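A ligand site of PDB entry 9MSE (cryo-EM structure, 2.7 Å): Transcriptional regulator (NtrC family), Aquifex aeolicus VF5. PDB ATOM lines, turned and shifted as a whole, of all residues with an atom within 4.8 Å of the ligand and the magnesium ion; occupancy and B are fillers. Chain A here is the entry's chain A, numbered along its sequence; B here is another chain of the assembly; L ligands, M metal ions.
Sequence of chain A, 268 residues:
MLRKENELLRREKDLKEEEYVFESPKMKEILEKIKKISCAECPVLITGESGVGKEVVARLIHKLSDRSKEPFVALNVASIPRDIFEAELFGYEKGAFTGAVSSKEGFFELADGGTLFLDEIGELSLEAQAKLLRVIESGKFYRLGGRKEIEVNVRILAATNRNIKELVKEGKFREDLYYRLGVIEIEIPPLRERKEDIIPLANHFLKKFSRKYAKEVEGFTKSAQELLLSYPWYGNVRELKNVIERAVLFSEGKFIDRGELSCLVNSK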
ATOM      1  N   TYR A  20      -3.778  -8.492  22.333  1.00  0.00           N
ATOM      2  CA  TYR A  20      -4.177  -7.721  23.505  1.00  0.00           C
ATOM      3  C   TYR A  20      -2.944  -7.388  24.340  1.00  0.00           C
ATOM      4  O   TYR A  20      -1.841  -7.899  24.091  1.00  0.00           O
ATOM      5  CB  TYR A  20      -5.201  -8.486  24.352  1.00  0.00           C
ATOM      6  CG  TYR A  20      -6.401  -8.948  23.557  1.00  0.00           C
ATOM      7  CD1 TYR A  20      -7.442  -8.076  23.275  1.00  0.00           C
ATOM      8  CD2 TYR A  20      -6.492 -10.250  23.094  1.00  0.00           C
ATOM      9  CE1 TYR A  20      -8.541  -8.491  22.548  1.00  0.00           C
ATOM     10  CE2 TYR A  20      -7.592 -10.672  22.375  1.00  0.00           C
ATOM     11  CZ  TYR A  20      -8.617  -9.793  22.102  1.00  0.00           C
ATOM     12  OH  TYR A  20      -9.709 -10.211  21.387  1.00  0.00           O
ATOM     13  N   VAL A  21      -3.129  -6.516  25.324  1.00  0.00           N
ATOM     14  CA  VAL A  21      -2.057  -6.007  26.162  1.00  0.00           C
ATOM     15  C   VAL A  21      -2.299  -6.466  27.592  1.00  0.00           C
ATOM     16  O   VAL A  21      -3.345  -6.150  28.176  1.00  0.00           O
ATOM     17  CB  VAL A  21      -1.946  -4.473  26.086  1.00  0.00           C
ATOM     18  CG1 VAL A  21      -1.008  -3.953  27.160  1.00  0.00           C
ATOM     19  CG2 VAL A  21      -1.470  -4.048  24.703  1.00  0.00           C
ATOM     20  N   PHE A  22      -1.327  -7.189  28.156  1.00  0.00           N
ATOM     21  CA  PHE A  22      -1.355  -7.623  29.550  1.00  0.00           C
ATOM     22  C   PHE A  22       0.034  -7.365  30.127  1.00  0.00           C
ATOM     23  O   PHE A  22       0.893  -8.244  30.119  1.00  0.00           O
ATOM     24  CB  PHE A  22      -1.749  -9.087  29.670  1.00  0.00           C
ATOM     25  CG  PHE A  22      -3.171  -9.369  29.298  1.00  0.00           C
ATOM     26  CD1 PHE A  22      -4.180  -9.315  30.245  1.00  0.00           C
ATOM     27  CD2 PHE A  22      -3.512  -9.684  27.988  1.00  0.00           C
ATOM     28  CE1 PHE A  22      -5.492  -9.573  29.903  1.00  0.00           C
ATOM     29  CE2 PHE A  22      -4.823  -9.935  27.638  1.00  0.00           C
ATOM     30  CZ  PHE A  22      -5.816  -9.880  28.602  1.00  0.00           C
ATOM     31  N   GLU A  49     -15.911  -2.192  35.637  1.00  0.00           N
ATOM     32  CA  GLU A  49     -16.526  -0.953  35.194  1.00  0.00           C
ATOM     33  C   GLU A  49     -16.761  -1.022  33.682  1.00  0.00           C
ATOM     34  O   GLU A  49     -16.644  -2.082  33.063  1.00  0.00           O
ATOM     35  CB  GLU A  49     -15.667   0.245  35.582  1.00  0.00           C
ATOM     36  CG  GLU A  49     -15.411   0.386  37.082  1.00  0.00           C
ATOM     37  CD  GLU A  49     -16.640   0.849  37.839  1.00  0.00           C
ATOM     38  OE1 GLU A  49     -17.641   1.234  37.198  1.00  0.00           O
ATOM     39  OE2 GLU A  49     -16.607   0.825  39.086  1.00  0.00           O
ATOM     40  N   SER A  50     -17.096   0.110  33.083  1.00  0.00           N
ATOM     41  CA  SER A  50     -17.293   0.166  31.632  1.00  0.00           C
ATOM     42  C   SER A  50     -15.945   0.165  30.928  1.00  0.00           C
ATOM     43  O   SER A  50     -15.047   0.929  31.272  1.00  0.00           O
ATOM     44  CB  SER A  50     -18.089   1.407  31.255  1.00  0.00           C
ATOM     45  OG  SER A  50     -18.215   1.518  29.849  1.00  0.00           O
ATOM     46  N   GLY A  51     -15.817  -0.697  29.923  1.00  0.00           N
ATOM     47  CA  GLY A  51     -14.601  -0.755  29.125  1.00  0.00           C
ATOM     48  C   GLY A  51     -13.377  -1.188  29.886  1.00  0.00           C
ATOM     49  O   GLY A  51     -12.307  -0.587  29.750  1.00  0.00           O
ATOM     50  N   VAL A  52     -13.499  -2.244  30.687  1.00  0.00           N
ATOM     51  CA  VAL A  52     -12.374  -2.752  31.466  1.00  0.00           C
ATOM     52  C   VAL A  52     -11.749  -3.945  30.760  1.00  0.00           C
ATOM     53  O   VAL A  52     -10.557  -4.232  30.934  1.00  0.00           O
ATOM     54  CB  VAL A  52     -12.814  -3.131  32.898  1.00  0.00           C
ATOM     55  CG1 VAL A  52     -13.151  -1.880  33.692  1.00  0.00           C
ATOM     56  CG2 VAL A  52     -13.997  -4.071  32.863  1.00  0.00           C
ATOM     57  N   GLY A  53     -12.525  -4.636  29.934  1.00  0.00           N
ATOM     58  CA  GLY A  53     -12.010  -5.767  29.187  1.00  0.00           C
ATOM     59  C   GLY A  53     -12.751  -7.067  29.419  1.00  0.00           C
ATOM     60  O   GLY A  53     -12.185  -8.148  29.245  1.00  0.00           O
ATOM     61  N   LYS A  54     -14.030  -6.976  29.800  1.00  0.00           N
ATOM     62  CA  LYS A  54     -14.802  -8.182  30.085  1.00  0.00           C
ATOM     63  C   LYS A  54     -14.979  -9.049  28.845  1.00  0.00           C
ATOM     64  O   LYS A  54     -14.862 -10.280  28.912  1.00  0.00           O
ATOM     65  CB  LYS A  54     -16.153  -7.787  30.679  1.00  0.00           C
ATOM     66  CG  LYS A  54     -16.036  -7.176  32.055  1.00  0.00           C
ATOM     67  CD  LYS A  54     -17.367  -6.679  32.568  1.00  0.00           C
ATOM     68  CE  LYS A  54     -17.753  -5.374  31.901  1.00  0.00           C
ATOM     69  NZ  LYS A  54     -18.969  -4.787  32.527  1.00  0.00           N
ATOM     70  N   GLU A  55     -15.261  -8.425  27.691  1.00  0.00           N
ATOM     71  CA  GLU A  55     -15.370  -9.182  26.453  1.00  0.00           C
ATOM     72  C   GLU A  55     -14.054  -9.863  26.108  1.00  0.00           C
ATOM     73  O   GLU A  55     -14.036 -11.017  25.674  1.00  0.00           O
ATOM     74  CB  GLU A  55     -15.812  -8.254  25.318  1.00  0.00           C
ATOM     75  CG  GLU A  55     -16.033  -8.940  23.990  1.00  0.00           C
ATOM     76  CD  GLU A  55     -17.434  -9.485  23.836  1.00  0.00           C
ATOM     77  OE1 GLU A  55     -18.275  -9.219  24.723  1.00  0.00           O
ATOM     78  OE2 GLU A  55     -17.694 -10.175  22.833  1.00  0.00           O
ATOM     79  N   VAL A  56     -12.942  -9.151  26.293  1.00  0.00           N
ATOM     80  CA  VAL A  56     -11.625  -9.733  26.051  1.00  0.00           C
ATOM     81  C   VAL A  56     -11.399 -10.927  26.971  1.00  0.00           C
ATOM     82  O   VAL A  56     -10.894 -11.973  26.527  1.00  0.00           O
ATOM     83  CB  VAL A  56     -10.541  -8.665  26.244  1.00  0.00           C
ATOM     84  CG1 VAL A  56      -9.161  -9.275  26.048  1.00  0.00           C
ATOM     85  CG2 VAL A  56     -10.745  -7.513  25.282  1.00  0.00           C
ATOM     86  N   ASP A 119     -24.193 -11.160  27.904  1.00  0.00           N
ATOM     87  CA  ASP A 119     -23.741  -9.837  28.303  1.00  0.00           C
ATOM     88  C   ASP A 119     -24.813  -9.102  29.090  1.00  0.00           C
ATOM     89  O   ASP A 119     -26.008  -9.241  28.833  1.00  0.00           O
ATOM     90  CB  ASP A 119     -23.353  -9.012  27.072  1.00  0.00           C
ATOM     91  CG  ASP A 119     -21.869  -9.033  26.800  1.00  0.00           C
ATOM     92  OD1 ASP A 119     -21.372 -10.079  26.327  1.00  0.00           O
ATOM     93  OD2 ASP A 119     -21.205  -8.006  27.046  1.00  0.00           O
ATOM     94  N   ASN A 161     -21.675  -4.735  34.549  1.00  0.00           N
ATOM     95  CA  ASN A 161     -20.995  -3.617  35.178  1.00  0.00           C
ATOM     96  C   ASN A 161     -21.694  -3.125  36.437  1.00  0.00           C
ATOM     97  O   ASN A 161     -21.066  -2.412  37.235  1.00  0.00           O
ATOM     98  CB  ASN A 161     -20.864  -2.445  34.195  1.00  0.00           C
ATOM     99  CG  ASN A 161     -22.193  -2.010  33.605  1.00  0.00           C
ATOM    100  OD1 ASN A 161     -23.256  -2.491  34.009  1.00  0.00           O
ATOM    101  ND2 ASN A 161     -22.142  -1.092  32.642  1.00  0.00           N
ATOM    102  N   ARG A 194      -4.502   0.914  37.293  1.00  0.00           N
ATOM    103  CA  ARG A 194      -3.567   0.208  36.429  1.00  0.00           C
ATOM    104  C   ARG A 194      -2.697   1.184  35.651  1.00  0.00           C
ATOM    105  O   ARG A 194      -2.515   1.052  34.440  1.00  0.00           O
ATOM    106  CB  ARG A 194      -4.310  -0.717  35.478  1.00  0.00           C
ATOM    107  CG  ARG A 194      -5.244  -1.703  36.157  1.00  0.00           C
ATOM    108  CD  ARG A 194      -6.352  -2.146  35.213  1.00  0.00           C
ATOM    109  NE  ARG A 194      -5.822  -2.707  33.977  1.00  0.00           N
ATOM    110  CZ  ARG A 194      -6.563  -3.060  32.941  1.00  0.00           C
ATOM    111  NH1 ARG A 194      -7.887  -2.923  32.950  1.00  0.00           N
ATOM    112  NH2 ARG A 194      -5.977  -3.569  31.862  1.00  0.00           N
ATOM    113  N   LEU A 201      -0.747   0.581  26.516  1.00  0.00           N
ATOM    114  CA  LEU A 201      -1.996   0.548  25.761  1.00  0.00           C
ATOM    115  C   LEU A 201      -2.010   1.610  24.670  1.00  0.00           C
ATOM    116  O   LEU A 201      -2.311   1.321  23.505  1.00  0.00           O
ATOM    117  CB  LEU A 201      -3.184   0.729  26.702  1.00  0.00           C
ATOM    118  CG  LEU A 201      -3.669  -0.502  27.450  1.00  0.00           C
ATOM    119  CD1 LEU A 201      -4.781  -0.140  28.424  1.00  0.00           C
ATOM    120  CD2 LEU A 201      -4.134  -1.552  26.468  1.00  0.00           C
ATOM    121  N   HIS A 204      -0.069   0.932  21.660  1.00  0.00           N
ATOM    122  CA  HIS A 204      -0.757  -0.138  20.936  1.00  0.00           C
ATOM    123  C   HIS A 204      -1.868   0.422  20.067  1.00  0.00           C
ATOM    124  O   HIS A 204      -2.031   0.010  18.910  1.00  0.00           O
ATOM    125  CB  HIS A 204      -1.313  -1.154  21.932  1.00  0.00           C
ATOM    126  CG  HIS A 204      -2.191  -2.191  21.305  1.00  0.00           C
ATOM    127  ND1 HIS A 204      -3.562  -2.034  21.204  1.00  0.00           N
ATOM    128  CD2 HIS A 204      -1.906  -3.386  20.741  1.00  0.00           C
ATOM    129  CE1 HIS A 204      -4.078  -3.104  20.602  1.00  0.00           C
ATOM    130  NE2 HIS A 204      -3.094  -3.932  20.320  1.00  0.00           N
ATOM    131  N   PHE A 205      -2.642   1.362  20.604  1.00  0.00           N
ATOM    132  CA  PHE A 205      -3.647   2.038  19.774  1.00  0.00           C
ATOM    133  C   PHE A 205      -2.983   2.936  18.747  1.00  0.00           C
ATOM    134  O   PHE A 205      -3.414   2.980  17.589  1.00  0.00           O
ATOM    135  CB  PHE A 205      -4.593   2.835  20.660  1.00  0.00           C
ATOM    136  CG  PHE A 205      -5.428   1.994  21.580  1.00  0.00           C
ATOM    137  CD1 PHE A 205      -5.915   0.762  21.159  1.00  0.00           C
ATOM    138  CD2 PHE A 205      -5.719   2.413  22.868  1.00  0.00           C
ATOM    139  CE1 PHE A 205      -6.678  -0.023  21.995  1.00  0.00           C
ATOM    140  CE2 PHE A 205      -6.482   1.627  23.704  1.00  0.00           C
ATOM    141  CZ  PHE A 205      -6.961   0.414  23.273  1.00  0.00           C
ATOM    142  N   LYS A 208      -1.994   1.196  15.744  1.00  0.00           N
ATOM    143  CA  LYS A 208      -3.117   0.620  15.008  1.00  0.00           C
ATOM    144  C   LYS A 208      -3.804   1.660  14.137  1.00  0.00           C
ATOM    145  O   LYS A 208      -4.060   1.413  12.946  1.00  0.00           O
ATOM    146  CB  LYS A 208      -4.119  -0.002  15.989  1.00  0.00           C
ATOM    147  CG  LYS A 208      -5.345  -0.572  15.312  1.00  0.00           C
ATOM    148  CD  LYS A 208      -6.209  -1.366  16.280  1.00  0.00           C
ATOM    149  CE  LYS A 208      -6.719  -0.486  17.416  1.00  0.00           C
ATOM    150  NZ  LYS A 208      -7.595  -1.243  18.350  1.00  0.00           N
ATOM    151  N   VAL A 237     -10.625   1.788  29.194  1.00  0.00           N
ATOM    152  CA  VAL A 237      -9.869   1.562  27.968  1.00  0.00           C
ATOM    153  C   VAL A 237     -10.573   2.187  26.768  1.00  0.00           C
ATOM    154  O   VAL A 237      -9.920   2.700  25.845  1.00  0.00           O
ATOM    155  CB  VAL A 237      -9.623   0.061  27.762  1.00  0.00           C
ATOM    156  CG1 VAL A 237      -8.718  -0.171  26.567  1.00  0.00           C
ATOM    157  CG2 VAL A 237      -9.014  -0.548  29.019  1.00  0.00           C
ATOM    158  N   ARG A 238     -11.911   2.132  26.737  1.00  0.00           N
ATOM    159  CA  ARG A 238     -12.637   2.651  25.583  1.00  0.00           C
ATOM    160  C   ARG A 238     -12.413   4.155  25.410  1.00  0.00           C
ATOM    161  O   ARG A 238     -12.216   4.637  24.290  1.00  0.00           O
ATOM    162  CB  ARG A 238     -14.126   2.340  25.711  1.00  0.00           C
ATOM    163  CG  ARG A 238     -14.946   2.853  24.547  1.00  0.00           C
ATOM    164  CD  ARG A 238     -16.418   2.504  24.680  1.00  0.00           C
ATOM    165  NE  ARG A 238     -16.682   1.083  24.504  1.00  0.00           N
ATOM    166  CZ  ARG A 238     -17.084   0.268  25.472  1.00  0.00           C
ATOM    167  NH1 ARG A 238     -17.277   0.710  26.701  1.00  0.00           N
ATOM    168  NH2 ARG A 238     -17.297  -1.009  25.189  1.00  0.00           N
ATOM    169  N   LYS A 241      -8.979   4.724  23.994  1.00  0.00           N
ATOM    170  CA  LYS A 241      -8.953   4.425  22.574  1.00  0.00           C
ATOM    171  C   LYS A 241      -9.585   5.552  21.768  1.00  0.00           C
ATOM    172  O   LYS A 241      -9.074   5.936  20.704  1.00  0.00           O
ATOM    173  CB  LYS A 241      -9.669   3.102  22.293  1.00  0.00           C
ATOM    174  CG  LYS A 241      -9.513   2.613  20.868  1.00  0.00           C
ATOM    175  CD  LYS A 241     -10.401   1.415  20.592  1.00  0.00           C
ATOM    176  CE  LYS A 241     -11.864   1.795  20.617  1.00  0.00           C
ATOM    177  NZ  LYS A 241     -12.727   0.687  20.133  1.00  0.00           N
ATOM    178  N   GLU B 137     -21.198  -1.054  18.716  1.00  0.00           N
ATOM    179  CA  GLU B 137     -19.770  -1.304  18.868  1.00  0.00           C
ATOM    180  C   GLU B 137     -19.258  -2.305  17.838  1.00  0.00           C
ATOM    181  O   GLU B 137     -18.267  -2.032  17.142  1.00  0.00           O
ATOM    182  CB  GLU B 137     -19.474  -1.797  20.288  1.00  0.00           C
ATOM    183  CG  GLU B 137     -18.011  -1.690  20.683  1.00  0.00           C
ATOM    184  CD  GLU B 137     -17.775  -2.074  22.127  1.00  0.00           C
ATOM    185  OE1 GLU B 137     -18.373  -3.061  22.590  1.00  0.00           O
ATOM    186  OE2 GLU B 137     -16.991  -1.373  22.805  1.00  0.00           O
ATOM    187  N   ASP B 176     -22.366   3.747  29.565  1.00  0.00           N
ATOM    188  CA  ASP B 176     -21.756   2.840  28.608  1.00  0.00           C
ATOM    189  C   ASP B 176     -22.202   3.104  27.174  1.00  0.00           C
ATOM    190  O   ASP B 176     -21.557   2.601  26.248  1.00  0.00           O
ATOM    191  CB  ASP B 176     -22.069   1.389  28.990  1.00  0.00           C
ATOM    192  CG  ASP B 176     -23.481   1.218  29.484  1.00  0.00           C
ATOM    193  OD1 ASP B 176     -24.030   2.161  30.092  1.00  0.00           O
ATOM    194  OD2 ASP B 176     -24.070   0.128  29.277  1.00  0.00           O
ATOM    195  N   ARG B 180     -19.805   4.895  23.663  1.00  0.00           N
ATOM    196  CA  ARG B 180     -19.936   4.240  22.370  1.00  0.00           C
ATOM    197  C   ARG B 180     -20.333   5.234  21.293  1.00  0.00           C
ATOM    198  O   ARG B 180     -19.866   5.141  20.150  1.00  0.00           O
ATOM    199  CB  ARG B 180     -20.960   3.113  22.451  1.00  0.00           C
ATOM    200  CG  ARG B 180     -20.453   1.860  23.149  1.00  0.00           C
ATOM    201  CD  ARG B 180     -21.520   0.783  23.149  1.00  0.00           C
ATOM    202  NE  ARG B 180     -21.011  -0.482  23.662  1.00  0.00           N
ATOM    203  CZ  ARG B 180     -21.008  -0.828  24.947  1.00  0.00           C
ATOM    204  NH1 ARG B 180     -21.465  -0.010  25.877  1.00  0.00           N
ATOM    205  NH2 ARG B 180     -20.521  -2.013  25.297  1.00  0.00           N
HETATM  206  P1  LIG L   1     -19.347  -2.546  28.749  1.00  0.00           P
HETATM  207  O1  LIG L   1     -20.264  -3.100  27.714  1.00  0.00           O
HETATM  208  O2  LIG L   1     -19.450  -3.281  30.087  1.00  0.00           O
HETATM  209  O3  LIG L   1     -19.498  -1.044  28.990  1.00  0.00           O
HETATM  210  P2  LIG L   1     -16.690  -3.822  28.368  1.00  0.00           P
HETATM  211  O4  LIG L   1     -15.989  -3.810  29.667  1.00  0.00           O
HETATM  212  O5  LIG L   1     -17.321  -5.152  27.953  1.00  0.00           O
HETATM  213  O6  LIG L   1     -17.832  -2.739  28.301  1.00  0.00           O
HETATM  214  P3  LIG L   1     -14.867  -4.073  26.069  1.00  0.00           P
HETATM  215  O7  LIG L   1     -15.729  -4.746  25.071  1.00  0.00           O
HETATM  216  O8  LIG L   1     -13.878  -4.991  26.777  1.00  0.00           O
HETATM  217  O9  LIG L   1     -15.745  -3.368  27.180  1.00  0.00           O
HETATM  218  O10 LIG L   1     -14.068  -2.882  25.410  1.00  0.00           O
HETATM  219  C1  LIG L   1     -13.783  -2.863  24.001  1.00  0.00           C
HETATM  220  C2  LIG L   1     -12.387  -2.356  23.768  1.00  0.00           C
HETATM  221  O11 LIG L   1     -11.547  -2.709  24.884  1.00  0.00           O
HETATM  222  C3  LIG L   1     -11.702  -2.918  22.509  1.00  0.00           C
HETATM  223  O12 LIG L   1     -11.486  -1.900  21.543  1.00  0.00           O
HETATM  224  C4  LIG L   1     -10.394  -3.520  23.026  1.00  0.00           C
HETATM  225  O13 LIG L   1      -9.291  -3.180  22.189  1.00  0.00           O
HETATM  226  C5  LIG L   1     -10.237  -2.859  24.397  1.00  0.00           C
HETATM  227  N1  LIG L   1      -9.470  -3.640  25.353  1.00  0.00           N
HETATM  228  C6  LIG L   1      -9.935  -4.244  26.492  1.00  0.00           C
HETATM  229  N2  LIG L   1      -9.019  -4.877  27.175  1.00  0.00           N
HETATM  230  C7  LIG L   1      -7.860  -4.673  26.431  1.00  0.00           C
HETATM  231  C8  LIG L   1      -6.523  -5.086  26.625  1.00  0.00           C
HETATM  232  N3  LIG L   1      -6.110  -5.827  27.664  1.00  0.00           N
HETATM  233  N4  LIG L   1      -5.612  -4.704  25.708  1.00  0.00           N
HETATM  234  C9  LIG L   1      -6.019  -3.969  24.664  1.00  0.00           C
HETATM  235  N5  LIG L   1      -7.243  -3.521  24.381  1.00  0.00           N
HETATM  236  C10 LIG L   1      -8.125  -3.904  25.313  1.00  0.00           C
HETATM  237 MG    MG M   1     -19.608  -5.665  27.430  1.00  0.00          MG
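Glu 49 touches the ligand (O to O4, 3.9 Å).
Glu 55 touches the ligand (CB to O7, 3.5 Å).
CG2 of Val 56 touches C6 of the ligand (3.6 Å).
Leu 201 touches the ligand.
CG1 of Val 237 touches N1 of the ligand, at 3.8 Å.
OE2 of Glu 137 of chain B touches C1 of the ligand (3.7 Å).
Asp 176 of chain B touches the ligand (CB to O3, 3.5 Å).
Hydrophobic or aromatic side chains that line the ligand: Val 21, Val 52, Val 56, Leu 201 and Val 237.
The nearest printed residue that does not touch the ligand is Tyr 20 (4.002 Å).
Asp 119 touches the magnesium ion (OD2 to MG, 2.9 Å).
The nearest printed residue that does not touch the magnesium ion is Arg 180 of chain B (4.3 Å).
The guanidinium group of Arg 180 of chain B is in salt-bridge range of an oxygen (O1) of the ligand, 2.7 Å away.
N of Val 21 sits at hydrogen-bond distance from N4 of the ligand.
O of Val 21 is in hydrogen-bond range of N3 of the ligand (2.8 Å).
NZ of Lys 54 is in salt-bridge range of O2 of the ligand (2.9 Å).
The side-chain hydroxyl of Ser 50 is in hydrogen-bond range of an oxygen (O3) of the ligand, 3.0 Å away.
An oxygen (O4) of the ligand lies within hydrogen-bond range of the backbone NH of Val 52 (3.1 Å).
N of Gly 51 lies within hydrogen-bond range of O4 of the ligand, 3.1 Å away.
The backbone NH (N) of Gly 53 sits close to an oxygen (O8) of the ligand (3.5 Å).
The side-chain amino group (NZ) of Lys 241 lies within hydrogen-bond range of an oxygen (O12) of the ligand, at 3.2 Å.
The guanidinium group (NH1) of Arg 238 is in salt-bridge range of an oxygen (O3) of the ligand (3.6 Å).
The magnesium ion is bound by an oxygen (O5) of the ligand (2.4 Å).
The magnesium ion has one donor atom within binding distance.
Slightly farther from the magnesium ion lies an oxygen (O1) of the ligand (2.7 Å).
The backbone carbonyl oxygen of Asp 176 of chain B is in hydrogen-bond range of the guanidinium group of Arg 180 of chain B (2.6 Å).
The side-chain carboxylate of Glu 137 of chain B is in salt-bridge range of the guanidinium group of Arg 180 of chain B (3.6 Å).
OG of Ser 50 lies within hydrogen-bond range of NH1 of Arg 238, 3.4 Å away.
O of Gly 51 is in hydrogen-bond range of N of Val 237 (3.0 Å).
The guanidinium group (NH2) of Arg 238 lies within salt-bridge range of the side-chain carboxylate (OE2) of Glu 137 of chain B (2.4 Å).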
